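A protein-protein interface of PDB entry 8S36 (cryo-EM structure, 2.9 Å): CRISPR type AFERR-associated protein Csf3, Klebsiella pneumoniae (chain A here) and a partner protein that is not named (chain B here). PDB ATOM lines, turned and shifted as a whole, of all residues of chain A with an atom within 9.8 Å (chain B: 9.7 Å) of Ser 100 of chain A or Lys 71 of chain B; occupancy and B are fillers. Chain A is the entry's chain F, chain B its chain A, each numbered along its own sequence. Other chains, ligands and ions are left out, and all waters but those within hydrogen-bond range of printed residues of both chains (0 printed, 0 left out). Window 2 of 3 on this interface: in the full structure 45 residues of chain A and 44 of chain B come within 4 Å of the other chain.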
ATOM      1  N   LYS A  93     -34.058  -1.461  26.335  1.00  0.00           N
ATOM      2  CA  LYS A  93     -33.393  -2.476  25.528  1.00  0.00           C
ATOM      3  C   LYS A  93     -32.458  -1.831  24.515  1.00  0.00           C
ATOM      4  O   LYS A  93     -31.391  -2.374  24.209  1.00  0.00           O
ATOM      5  CB  LYS A  93     -34.428  -3.343  24.813  1.00  0.00           C
ATOM      6  CG  LYS A  93     -34.994  -4.468  25.654  1.00  0.00           C
ATOM      7  CD  LYS A  93     -35.915  -5.352  24.831  1.00  0.00           C
ATOM      8  CE  LYS A  93     -36.519  -6.467  25.667  1.00  0.00           C
ATOM      9  NZ  LYS A  93     -37.368  -7.376  24.850  1.00  0.00           N
ATOM     10  N   LEU A  94     -32.847  -0.672  23.988  1.00  0.00           N
ATOM     11  CA  LEU A  94     -31.997   0.110  23.093  1.00  0.00           C
ATOM     12  C   LEU A  94     -31.203   1.141  23.895  1.00  0.00           C
ATOM     13  O   LEU A  94     -31.329   2.351  23.716  1.00  0.00           O
ATOM     14  CB  LEU A  94     -32.842   0.777  22.014  1.00  0.00           C
ATOM     15  CG  LEU A  94     -33.800  -0.133  21.242  1.00  0.00           C
ATOM     16  CD1 LEU A  94     -34.846   0.696  20.517  1.00  0.00           C
ATOM     17  CD2 LEU A  94     -33.032  -1.012  20.267  1.00  0.00           C
ATOM     18  N   SER A  95     -30.382   0.632  24.811  1.00  0.00           N
ATOM     19  CA  SER A  95     -29.574   1.477  25.675  1.00  0.00           C
ATOM     20  C   SER A  95     -28.203   0.847  25.857  1.00  0.00           C
ATOM     21  O   SER A  95     -28.039  -0.369  25.732  1.00  0.00           O
ATOM     22  CB  SER A  95     -30.239   1.682  27.042  1.00  0.00           C
ATOM     23  OG  SER A  95     -29.430   2.484  27.884  1.00  0.00           O
ATOM     24  N   THR A  96     -27.217   1.693  26.157  1.00  0.00           N
ATOM     25  CA  THR A  96     -25.860   1.210  26.369  1.00  0.00           C
ATOM     26  C   THR A  96     -25.701   0.472  27.690  1.00  0.00           C
ATOM     27  O   THR A  96     -24.666  -0.171  27.899  1.00  0.00           O
ATOM     28  CB  THR A  96     -24.877   2.381  26.319  1.00  0.00           C
ATOM     29  OG1 THR A  96     -25.262   3.286  25.279  1.00  0.00           O
ATOM     30  CG2 THR A  96     -23.461   1.885  26.057  1.00  0.00           C
ATOM     31  N   ALA A  97     -26.693   0.542  28.580  1.00  0.00           N
ATOM     32  CA  ALA A  97     -26.592  -0.174  29.846  1.00  0.00           C
ATOM     33  C   ALA A  97     -26.574  -1.682  29.637  1.00  0.00           C
ATOM     34  O   ALA A  97     -25.917  -2.401  30.399  1.00  0.00           O
ATOM     35  CB  ALA A  97     -27.750   0.217  30.762  1.00  0.00           C
ATOM     36  N   MET A  98     -27.277  -2.177  28.620  1.00  0.00           N
ATOM     37  CA  MET A  98     -27.377  -3.613  28.398  1.00  0.00           C
ATOM     38  C   MET A  98     -26.325  -4.145  27.439  1.00  0.00           C
ATOM     39  O   MET A  98     -25.872  -5.283  27.604  1.00  0.00           O
ATOM     40  CB  MET A  98     -28.757  -3.960  27.838  1.00  0.00           C
ATOM     41  CG  MET A  98     -29.894  -3.830  28.827  1.00  0.00           C
ATOM     42  SD  MET A  98     -31.415  -4.518  28.151  1.00  0.00           S
ATOM     43  CE  MET A  98     -32.057  -5.401  29.565  1.00  0.00           C
ATOM     44  N   PHE A  99     -25.928  -3.358  26.444  1.00  0.00           N
ATOM     45  CA  PHE A  99     -25.017  -3.842  25.418  1.00  0.00           C
ATOM     46  C   PHE A  99     -24.168  -2.692  24.904  1.00  0.00           C
ATOM     47  O   PHE A  99     -24.488  -1.518  25.104  1.00  0.00           O
ATOM     48  CB  PHE A  99     -25.782  -4.505  24.273  1.00  0.00           C
ATOM     49  CG  PHE A  99     -26.421  -3.538  23.324  1.00  0.00           C
ATOM     50  CD1 PHE A  99     -27.376  -2.640  23.764  1.00  0.00           C
ATOM     51  CD2 PHE A  99     -26.078  -3.541  21.985  1.00  0.00           C
ATOM     52  CE1 PHE A  99     -27.967  -1.754  22.888  1.00  0.00           C
ATOM     53  CE2 PHE A  99     -26.668  -2.661  21.105  1.00  0.00           C
ATOM     54  CZ  PHE A  99     -27.613  -1.765  21.557  1.00  0.00           C
ATOM     55  N   SER A 100     -23.073  -3.050  24.234  1.00  0.00           N
ATOM     56  CA  SER A 100     -22.187  -2.075  23.619  1.00  0.00           C
ATOM     57  C   SER A 100     -22.487  -2.021  22.126  1.00  0.00           C
ATOM     58  O   SER A 100     -21.972  -2.855  21.367  1.00  0.00           O
ATOM     59  CB  SER A 100     -20.723  -2.449  23.860  1.00  0.00           C
ATOM     60  OG  SER A 100     -19.854  -1.570  23.169  1.00  0.00           O
ATOM     61  N   PRO A 101     -23.297  -1.078  21.651  1.00  0.00           N
ATOM     62  CA  PRO A 101     -23.525  -0.970  20.207  1.00  0.00           C
ATOM     63  C   PRO A 101     -22.274  -0.494  19.492  1.00  0.00           C
ATOM     64  O   PRO A 101     -21.402   0.159  20.071  1.00  0.00           O
ATOM     65  CB  PRO A 101     -24.651   0.062  20.096  1.00  0.00           C
ATOM     66  CG  PRO A 101     -24.544   0.863  21.330  1.00  0.00           C
ATOM     67  CD  PRO A 101     -24.078  -0.076  22.399  1.00  0.00           C
ATOM     68  N   ARG A 102     -22.186  -0.839  18.211  1.00  0.00           N
ATOM     69  CA  ARG A 102     -21.073  -0.348  17.415  1.00  0.00           C
ATOM     70  C   ARG A 102     -21.145   1.170  17.349  1.00  0.00           C
ATOM     71  O   ARG A 102     -22.221   1.753  17.187  1.00  0.00           O
ATOM     72  CB  ARG A 102     -21.114  -0.946  16.009  1.00  0.00           C
ATOM     73  CG  ARG A 102     -19.762  -1.397  15.485  1.00  0.00           C
ATOM     74  CD  ARG A 102     -19.893  -2.062  14.124  1.00  0.00           C
ATOM     75  NE  ARG A 102     -20.662  -3.302  14.200  1.00  0.00           N
ATOM     76  CZ  ARG A 102     -21.604  -3.682  13.345  1.00  0.00           C
ATOM     77  NH1 ARG A 102     -21.926  -2.953  12.286  1.00  0.00           N
ATOM     78  NH2 ARG A 102     -22.241  -4.830  13.554  1.00  0.00           N
ATOM     79  N   THR A 103     -19.988   1.811  17.472  1.00  0.00           N
ATOM     80  CA  THR A 103     -19.902   3.254  17.635  1.00  0.00           C
ATOM     81  C   THR A 103     -19.163   3.875  16.461  1.00  0.00           C
ATOM     82  O   THR A 103     -18.179   3.317  15.968  1.00  0.00           O
ATOM     83  CB  THR A 103     -19.196   3.625  18.946  1.00  0.00           C
ATOM     84  OG1 THR A 103     -19.318   5.034  19.176  1.00  0.00           O
ATOM     85  CG2 THR A 103     -17.719   3.248  18.897  1.00  0.00           C
ATOM     86  N   ARG A 104     -19.645   5.036  16.025  1.00  0.00           N
ATOM     87  CA  ARG A 104     -18.943   5.857  15.048  1.00  0.00           C
ATOM     88  C   ARG A 104     -19.113   7.308  15.462  1.00  0.00           C
ATOM     89  O   ARG A 104     -20.244   7.779  15.623  1.00  0.00           O
ATOM     90  CB  ARG A 104     -19.488   5.635  13.633  1.00  0.00           C
ATOM     91  CG  ARG A 104     -19.449   4.190  13.162  1.00  0.00           C
ATOM     92  CD  ARG A 104     -19.120   4.091  11.681  1.00  0.00           C
ATOM     93  NE  ARG A 104     -19.957   4.965  10.868  1.00  0.00           N
ATOM     94  CZ  ARG A 104     -19.724   5.261   9.596  1.00  0.00           C
ATOM     95  NH1 ARG A 104     -18.680   4.767   8.950  1.00  0.00           N
ATOM     96  NH2 ARG A 104     -20.560   6.073   8.956  1.00  0.00           N
ATOM     97  N   GLY A 106     -18.630   8.765  18.222  1.00  0.00           N
ATOM     98  CA  GLY A 106     -19.396   8.808  19.450  1.00  0.00           C
ATOM     99  C   GLY A 106     -20.878   8.540  19.309  1.00  0.00           C
ATOM    100  O   GLY A 106     -21.572   8.471  20.330  1.00  0.00           O
ATOM    101  N   LEU A 107     -21.393   8.385  18.090  1.00  0.00           N
ATOM    102  CA  LEU A 107     -22.802   8.090  17.875  1.00  0.00           C
ATOM    103  C   LEU A 107     -23.000   6.581  17.836  1.00  0.00           C
ATOM    104  O   LEU A 107     -22.233   5.863  17.186  1.00  0.00           O
ATOM    105  CB  LEU A 107     -23.299   8.721  16.575  1.00  0.00           C
ATOM    106  CG  LEU A 107     -23.924  10.110  16.711  1.00  0.00           C
ATOM    107  CD1 LEU A 107     -22.849  11.164  16.916  1.00  0.00           C
ATOM    108  CD2 LEU A 107     -24.774  10.435  15.492  1.00  0.00           C
ATOM    109  N   PHE A 108     -24.029   6.108  18.530  1.00  0.00           N
ATOM    110  CA  PHE A 108     -24.321   4.684  18.615  1.00  0.00           C
ATOM    111  C   PHE A 108     -25.195   4.283  17.433  1.00  0.00           C
ATOM    112  O   PHE A 108     -26.275   4.848  17.230  1.00  0.00           O
ATOM    113  CB  PHE A 108     -25.009   4.355  19.938  1.00  0.00           C
ATOM    114  CG  PHE A 108     -24.165   4.643  21.149  1.00  0.00           C
ATOM    115  CD1 PHE A 108     -22.848   4.217  21.212  1.00  0.00           C
ATOM    116  CD2 PHE A 108     -24.688   5.344  22.220  1.00  0.00           C
ATOM    117  CE1 PHE A 108     -22.073   4.481  22.322  1.00  0.00           C
ATOM    118  CE2 PHE A 108     -23.915   5.611  23.333  1.00  0.00           C
ATOM    119  CZ  PHE A 108     -22.607   5.180  23.384  1.00  0.00           C
ATOM    120  N   THR A 109     -24.721   3.311  16.657  1.00  0.00           N
ATOM    121  CA  THR A 109     -25.410   2.880  15.448  1.00  0.00           C
ATOM    122  C   THR A 109     -26.777   2.307  15.786  1.00  0.00           C
ATOM    123  O   THR A 109     -26.875   1.254  16.424  1.00  0.00           O
ATOM    124  CB  THR A 109     -24.578   1.839  14.697  1.00  0.00           C
ATOM    125  OG1 THR A 109     -24.425   0.668  15.508  1.00  0.00           O
ATOM    126  CG2 THR A 109     -23.209   2.396  14.347  1.00  0.00           C
ATOM    127  N   VAL A 111     -30.283   0.423  15.830  1.00  0.00           N
ATOM    128  CA  VAL A 111     -30.706  -0.889  15.358  1.00  0.00           C
ATOM    129  C   VAL A 111     -31.772  -0.702  14.289  1.00  0.00           C
ATOM    130  O   VAL A 111     -32.725   0.062  14.473  1.00  0.00           O
ATOM    131  CB  VAL A 111     -31.228  -1.746  16.523  1.00  0.00           C
ATOM    132  CG1 VAL A 111     -31.409  -3.191  16.082  1.00  0.00           C
ATOM    133  CG2 VAL A 111     -30.285  -1.664  17.707  1.00  0.00           C
ATOM    134  N   HIS B  57     -32.688 -10.361  31.609  1.00  0.00           N
ATOM    135  CA  HIS B  57     -31.562  -9.790  30.883  1.00  0.00           C
ATOM    136  C   HIS B  57     -30.869  -8.713  31.705  1.00  0.00           C
ATOM    137  O   HIS B  57     -29.634  -8.615  31.705  1.00  0.00           O
ATOM    138  CB  HIS B  57     -32.037  -9.226  29.545  1.00  0.00           C
ATOM    139  CG  HIS B  57     -30.925  -8.872  28.610  1.00  0.00           C
ATOM    140  ND1 HIS B  57     -29.758  -9.602  28.529  1.00  0.00           N
ATOM    141  CD2 HIS B  57     -30.803  -7.869  27.708  1.00  0.00           C
ATOM    142  CE1 HIS B  57     -28.965  -9.061  27.623  1.00  0.00           C
ATOM    143  NE2 HIS B  57     -29.576  -8.008  27.109  1.00  0.00           N
ATOM    144  N   VAL B  61     -26.952  -8.852  32.852  1.00  0.00           N
ATOM    145  CA  VAL B  61     -25.968  -7.809  32.575  1.00  0.00           C
ATOM    146  C   VAL B  61     -25.360  -7.301  33.876  1.00  0.00           C
ATOM    147  O   VAL B  61     -24.145  -7.087  33.962  1.00  0.00           O
ATOM    148  CB  VAL B  61     -26.566  -6.666  31.728  1.00  0.00           C
ATOM    149  CG1 VAL B  61     -27.027  -7.191  30.371  1.00  0.00           C
ATOM    150  CG2 VAL B  61     -27.698  -5.982  32.436  1.00  0.00           C
ATOM    151  N   VAL B  64     -22.929  -9.907  35.180  1.00  0.00           N
ATOM    152  CA  VAL B  64     -21.711  -9.802  34.386  1.00  0.00           C
ATOM    153  C   VAL B  64     -21.013  -8.479  34.666  1.00  0.00           C
ATOM    154  O   VAL B  64     -19.786  -8.424  34.810  1.00  0.00           O
ATOM    155  CB  VAL B  64     -22.038  -9.968  32.892  1.00  0.00           C
ATOM    156  CG1 VAL B  64     -20.848  -9.568  32.034  1.00  0.00           C
ATOM    157  CG2 VAL B  64     -22.457 -11.401  32.598  1.00  0.00           C
ATOM    158  N   GLY B  65     -21.779  -7.398  34.744  1.00  0.00           N
ATOM    159  CA  GLY B  65     -21.216  -6.080  34.929  1.00  0.00           C
ATOM    160  C   GLY B  65     -20.669  -5.518  33.632  1.00  0.00           C
ATOM    161  O   GLY B  65     -20.943  -6.007  32.532  1.00  0.00           O
ATOM    162  N   LEU B  66     -19.871  -4.466  33.776  1.00  0.00           N
ATOM    163  CA  LEU B  66     -19.238  -3.799  32.650  1.00  0.00           C
ATOM    164  C   LEU B  66     -17.760  -4.158  32.587  1.00  0.00           C
ATOM    165  O   LEU B  66     -17.171  -4.646  33.556  1.00  0.00           O
ATOM    166  CB  LEU B  66     -19.403  -2.280  32.751  1.00  0.00           C
ATOM    167  CG  LEU B  66     -20.845  -1.774  32.700  1.00  0.00           C
ATOM    168  CD1 LEU B  66     -21.334  -1.404  34.091  1.00  0.00           C
ATOM    169  CD2 LEU B  66     -20.963  -0.589  31.755  1.00  0.00           C
ATOM    170  N   ASN B  67     -17.166  -3.908  31.425  1.00  0.00           N
ATOM    171  CA  ASN B  67     -15.741  -4.123  31.236  1.00  0.00           C
ATOM    172  C   ASN B  67     -14.948  -3.040  31.967  1.00  0.00           C
ATOM    173  O   ASN B  67     -15.502  -2.152  32.621  1.00  0.00           O
ATOM    174  CB  ASN B  67     -15.406  -4.141  29.747  1.00  0.00           C
ATOM    175  CG  ASN B  67     -15.922  -5.381  29.049  1.00  0.00           C
ATOM    176  OD1 ASN B  67     -15.968  -6.463  29.633  1.00  0.00           O
ATOM    177  ND2 ASN B  67     -16.314  -5.230  27.789  1.00  0.00           N
ATOM    178  N   ALA B  68     -13.622  -3.118  31.848  1.00  0.00           N
ATOM    179  CA  ALA B  68     -12.765  -2.060  32.369  1.00  0.00           C
ATOM    180  C   ALA B  68     -12.987  -0.746  31.635  1.00  0.00           C
ATOM    181  O   ALA B  68     -12.690   0.319  32.186  1.00  0.00           O
ATOM    182  CB  ALA B  68     -11.297  -2.474  32.270  1.00  0.00           C
ATOM    183  N   ASP B  69     -13.506  -0.800  30.410  1.00  0.00           N
ATOM    184  CA  ASP B  69     -13.776   0.387  29.612  1.00  0.00           C
ATOM    185  C   ASP B  69     -15.107   1.040  29.959  1.00  0.00           C
ATOM    186  O   ASP B  69     -15.432   2.086  29.389  1.00  0.00           O
ATOM    187  CB  ASP B  69     -13.754   0.023  28.123  1.00  0.00           C
ATOM    188  CG  ASP B  69     -13.641   1.240  27.223  1.00  0.00           C
ATOM    189  OD1 ASP B  69     -13.349   2.342  27.733  1.00  0.00           O
ATOM    190  OD2 ASP B  69     -13.844   1.093  25.999  1.00  0.00           O
ATOM    191  N   GLY B  70     -15.880   0.459  30.874  1.00  0.00           N
ATOM    192  CA  GLY B  70     -17.188   0.994  31.190  1.00  0.00           C
ATOM    193  C   GLY B  70     -18.248   0.718  30.154  1.00  0.00           C
ATOM    194  O   GLY B  70     -19.273   1.406  30.135  1.00  0.00           O
ATOM    195  N   LYS B  71     -18.034  -0.270  29.288  1.00  0.00           N
ATOM    196  CA  LYS B  71     -18.994  -0.657  28.268  1.00  0.00           C
ATOM    197  C   LYS B  71     -19.458  -2.084  28.523  1.00  0.00           C
ATOM    198  O   LYS B  71     -18.698  -2.923  29.014  1.00  0.00           O
ATOM    199  CB  LYS B  71     -18.389  -0.553  26.864  1.00  0.00           C
ATOM    200  CG  LYS B  71     -17.999   0.856  26.459  1.00  0.00           C
ATOM    201  CD  LYS B  71     -17.459   0.889  25.038  1.00  0.00           C
ATOM    202  CE  LYS B  71     -16.969   2.277  24.657  1.00  0.00           C
ATOM    203  NZ  LYS B  71     -18.038   3.306  24.778  1.00  0.00           N
ATOM    204  N   SER B  72     -20.714  -2.346  28.185  1.00  0.00           N
ATOM    205  CA  SER B  72     -21.272  -3.672  28.395  1.00  0.00           C
ATOM    206  C   SER B  72     -20.545  -4.685  27.512  1.00  0.00           C
ATOM    207  O   SER B  72     -20.278  -4.400  26.338  1.00  0.00           O
ATOM    208  CB  SER B  72     -22.767  -3.677  28.078  1.00  0.00           C
ATOM    209  OG  SER B  72     -23.432  -2.614  28.737  1.00  0.00           O
ATOM    210  N   PRO B  73     -20.209  -5.874  28.027  1.00  0.00           N
ATOM    211  CA  PRO B  73     -19.499  -6.848  27.181  1.00  0.00           C
ATOM    212  C   PRO B  73     -20.331  -7.376  26.028  1.00  0.00           C
ATOM    213  O   PRO B  73     -19.761  -7.941  25.088  1.00  0.00           O
ATOM    214  CB  PRO B  73     -19.138  -7.977  28.158  1.00  0.00           C
ATOM    215  CG  PRO B  73     -19.244  -7.382  29.504  1.00  0.00           C
ATOM    216  CD  PRO B  73     -20.317  -6.353  29.417  1.00  0.00           C
ATOM    217  N   PHE B  74     -21.651  -7.215  26.064  1.00  0.00           N
ATOM    218  CA  PHE B  74     -22.509  -7.769  25.027  1.00  0.00           C
ATOM    219  C   PHE B  74     -22.554  -6.841  23.823  1.00  0.00           C
ATOM    220  O   PHE B  74     -22.702  -5.623  23.967  1.00  0.00           O
ATOM    221  CB  PHE B  74     -23.921  -7.987  25.566  1.00  0.00           C
ATOM    222  CG  PHE B  74     -23.958  -8.699  26.881  1.00  0.00           C
ATOM    223  CD1 PHE B  74     -23.685 -10.050  26.953  1.00  0.00           C
ATOM    224  CD2 PHE B  74     -24.260  -8.018  28.046  1.00  0.00           C
ATOM    225  CE1 PHE B  74     -23.717 -10.710  28.158  1.00  0.00           C
ATOM    226  CE2 PHE B  74     -24.292  -8.675  29.257  1.00  0.00           C
ATOM    227  CZ  PHE B  74     -24.020 -10.024  29.313  1.00  0.00           C
ATOM    228  N   ASP B  75     -22.428  -7.422  22.633  1.00  0.00           N
ATOM    229  CA  ASP B  75     -22.578  -6.687  21.389  1.00  0.00           C
ATOM    230  C   ASP B  75     -24.039  -6.756  20.950  1.00  0.00           C
ATOM    231  O   ASP B  75     -24.911  -7.219  21.689  1.00  0.00           O
ATOM    232  CB  ASP B  75     -21.629  -7.243  20.329  1.00  0.00           C
ATOM    233  CG  ASP B  75     -21.939  -8.681  19.962  1.00  0.00           C
ATOM    234  OD1 ASP B  75     -22.724  -9.330  20.688  1.00  0.00           O
ATOM    235  OD2 ASP B  75     -21.398  -9.166  18.947  1.00  0.00           O
ATOM    236  N   LEU B  76     -24.325  -6.293  19.732  1.00  0.00           N
ATOM    237  CA  LEU B  76     -25.700  -6.334  19.243  1.00  0.00           C
ATOM    238  C   LEU B  76     -26.184  -7.770  19.083  1.00  0.00           C
ATOM    239  O   LEU B  76     -27.330  -8.086  19.422  1.00  0.00           O
ATOM    240  CB  LEU B  76     -25.807  -5.582  17.917  1.00  0.00           C
ATOM    241  CG  LEU B  76     -27.231  -5.327  17.418  1.00  0.00           C
ATOM    242  CD1 LEU B  76     -27.931  -4.289  18.281  1.00  0.00           C
ATOM    243  CD2 LEU B  76     -27.216  -4.893  15.962  1.00  0.00           C
ATOM    244  N   ALA B  77     -25.327  -8.654  18.571  1.00  0.00           N
ATOM    245  CA  ALA B  77     -25.744 -10.035  18.343  1.00  0.00           C
ATOM    246  C   ALA B  77     -26.060 -10.737  19.656  1.00  0.00           C
ATOM    247  O   ALA B  77     -27.122 -11.354  19.802  1.00  0.00           O
ATOM    248  CB  ALA B  77     -24.657 -10.788  17.577  1.00  0.00           C
ATOM    249  N   GLU B  78     -25.158 -10.640  20.632  1.00  0.00           N
ATOM    250  CA  GLU B  78     -25.416 -11.257  21.928  1.00  0.00           C
ATOM    251  C   GLU B  78     -26.602 -10.597  22.618  1.00  0.00           C
ATOM    252  O   GLU B  78     -27.410 -11.272  23.268  1.00  0.00           O
ATOM    253  CB  GLU B  78     -24.169 -11.176  22.808  1.00  0.00           C
ATOM    254  CG  GLU B  78     -23.032 -12.070  22.344  1.00  0.00           C
ATOM    255  CD  GLU B  78     -21.670 -11.428  22.516  1.00  0.00           C
ATOM    256  OE1 GLU B  78     -21.460 -10.740  23.538  1.00  0.00           O
ATOM    257  OE2 GLU B  78     -20.809 -11.613  21.632  1.00  0.00           O
ATOM    258  N   HIS B  79     -26.712  -9.274  22.501  1.00  0.00           N
ATOM    259  CA  HIS B  79     -27.824  -8.578  23.133  1.00  0.00           C
ATOM    260  C   HIS B  79     -29.160  -9.052  22.583  1.00  0.00           C
ATOM    261  O   HIS B  79     -30.109  -9.270  23.344  1.00  0.00           O
ATOM    262  CB  HIS B  79     -27.672  -7.074  22.928  1.00  0.00           C
ATOM    263  CG  HIS B  79     -28.842  -6.275  23.413  1.00  0.00           C
ATOM    264  ND1 HIS B  79     -28.954  -5.833  24.714  1.00  0.00           N
ATOM    265  CD2 HIS B  79     -29.950  -5.835  22.771  1.00  0.00           C
ATOM    266  CE1 HIS B  79     -30.081  -5.158  24.852  1.00  0.00           C
ATOM    267  NE2 HIS B  79     -30.704  -5.144  23.688  1.00  0.00           N
ATOM    268  N   PHE B  80     -29.260  -9.215  21.261  1.00  0.00           N
ATOM    269  CA  PHE B  80     -30.516  -9.690  20.691  1.00  0.00           C
ATOM    270  C   PHE B  80     -30.729 -11.171  20.967  1.00  0.00           C
ATOM    271  O   PHE B  80     -31.876 -11.620  21.068  1.00  0.00           O
ATOM    272  CB  PHE B  80     -30.558  -9.430  19.183  1.00  0.00           C
ATOM    273  CG  PHE B  80     -31.432  -8.267  18.784  1.00  0.00           C
ATOM    274  CD1 PHE B  80     -31.492  -7.115  19.556  1.00  0.00           C
ATOM    275  CD2 PHE B  80     -32.226  -8.346  17.655  1.00  0.00           C
ATOM    276  CE1 PHE B  80     -32.300  -6.058  19.189  1.00  0.00           C
ATOM    277  CE2 PHE B  80     -33.041  -7.294  17.288  1.00  0.00           C
ATOM    278  CZ  PHE B  80     -33.078  -6.149  18.056  1.00  0.00           C
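The side-chain hydroxyl (OG) of Ser 72 of chain B is in hydrogen-bond range of the backbone NH (N) of Phe 99 of chain A (3.5 Å).
The backbone NH (N) of Ser 100 of chain A is in hydrogen-bond range of the backbone carbonyl oxygen (O) of Phe 74 of chain B, at 2.6 Å.
O of Lys 93 of chain A sits at hydrogen-bond distance from NE2 of His 79 of chain B (2.9 Å).
The side-chain hydroxyl (OG) of Ser 72 of chain B sits at hydrogen-bond distance from the backbone carbonyl oxygen (O) of Thr 96 of chain A.
OG of Ser 72 of chain B lies within hydrogen-bond range of O of Ala 97 of chain A, 3.0 Å away.
The side-chain hydroxyl (OG) of Ser 95 of chain A sits close to the backbone NH (N) of Ala 97 of chain A (3.4 Å).
The side-chain carboxylate of Asp 75 of chain B sits close to the backbone NH of Ala 77 of chain B (3.4 Å).
NE2 of His 57 of chain B sits at hydrogen-bond distance from ND1 of His 79 of chain B.
OD1 of Asp 75 of chain B sits at hydrogen-bond distance from N of Glu 78 of chain B (2.8 Å).
Among the printed residues, merely in contact across the chains: Met 98 of chain A with His 57 of chain B, Met 98 of chain A with Val 61 of chain B, Met 98 of chain A with Ser 72 of chain B, Met 98 of chain A with Phe 74 of chain B, Met 98 of chain A with His 79 of chain B, Phe 99 of chain A with Phe 74 of chain B, Phe 99 of chain A with Asp 75 of chain B, Phe 99 of chain A with Leu 76 of chain B, Phe 99 of chain A with His 79 of chain B, Ser 100 of chain A with Lys 71 of chain B, Ser 100 of chain A with Ser 72 of chain B, Ser 100 of chain A with Asp 75 of chain B, Val 111 of chain A with Leu 76 of chain B and Val 111 of chain A with Phe 80 of chain B.
Printed residues of chain B within 4 Å of Met 98 of chain A: His 57 (3.3 Å), Val 61 (3.6 Å), Ser 72 (3.5 Å), Phe 74 (3.2 Å) and His 79 (3.5 Å).
Phe 99 of chain A touches just these residues of chain B: Ser 72 (3.5 Å), Phe 74 (3.3 Å), Asp 75 (3.8 Å), Leu 76 (3.5 Å) and His 79 (3.5 Å).
Ser 100 of chain A touches just these residues of chain B: Lys 71 (3.9 Å), Ser 72 (3.2 Å), Phe 74 (2.6 Å) and Asp 75 (3.9 Å).
No residue of chain B comes within 4 Å of Pro 101 of chain A.
Ala 68 of chain B touches none of the printed residues of chain A.
No residue of chain A comes within 4 Å of Asp 69 of chain B.
Of chain A, only Ser 100 (3.9 Å) comes within 4 Å of Lys 71 of chain B.
Of the printed residues of chain A, Ser 72 of chain B touches Thr 96, Ala 97, Met 98, Phe 99 and Ser 100.
No residue of chain A comes within 4 Å of Pro 73 of chain B.
Printed residues of chain A within 4 Å of Phe 74 of chain B: Met 98, Phe 99 and Ser 100.
Of the printed residues of chain A, Asp 75 of chain B touches Phe 99 (3.8 Å) and Ser 100 (3.9 Å).
Ala 77 of chain B touches none of the printed residues of chain A.
The nearest residue of chain B that does not touch Ser 100 of chain A is Leu 76 of chain B (4.5 Å).
The nearest printed residue of chain A that does not touch Leu 76 of chain B is Ser 100 of chain A (4.5 Å).
Of the 19 printed residues of chain B, 9 touch a printed residue of chain A.
Printed residues of chain B that touch a printed residue of chain A: His 57, Val 61, Lys 71, Ser 72, Phe 74, Asp 75, Leu 76, His 79 and Phe 80.
Hydrophobic or aromatic side chains of chain B within 4 Å of the printed part of chain A: His 57, Val 61, Phe 74, Leu 76, His 79 and Phe 80.
Hydrophobic or aromatic side chains of chain A within 4 Å of the printed part of chain B: Met 98, Phe 99 and Val 111.
Among the printed residues, 19 pairs touch across the chains.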
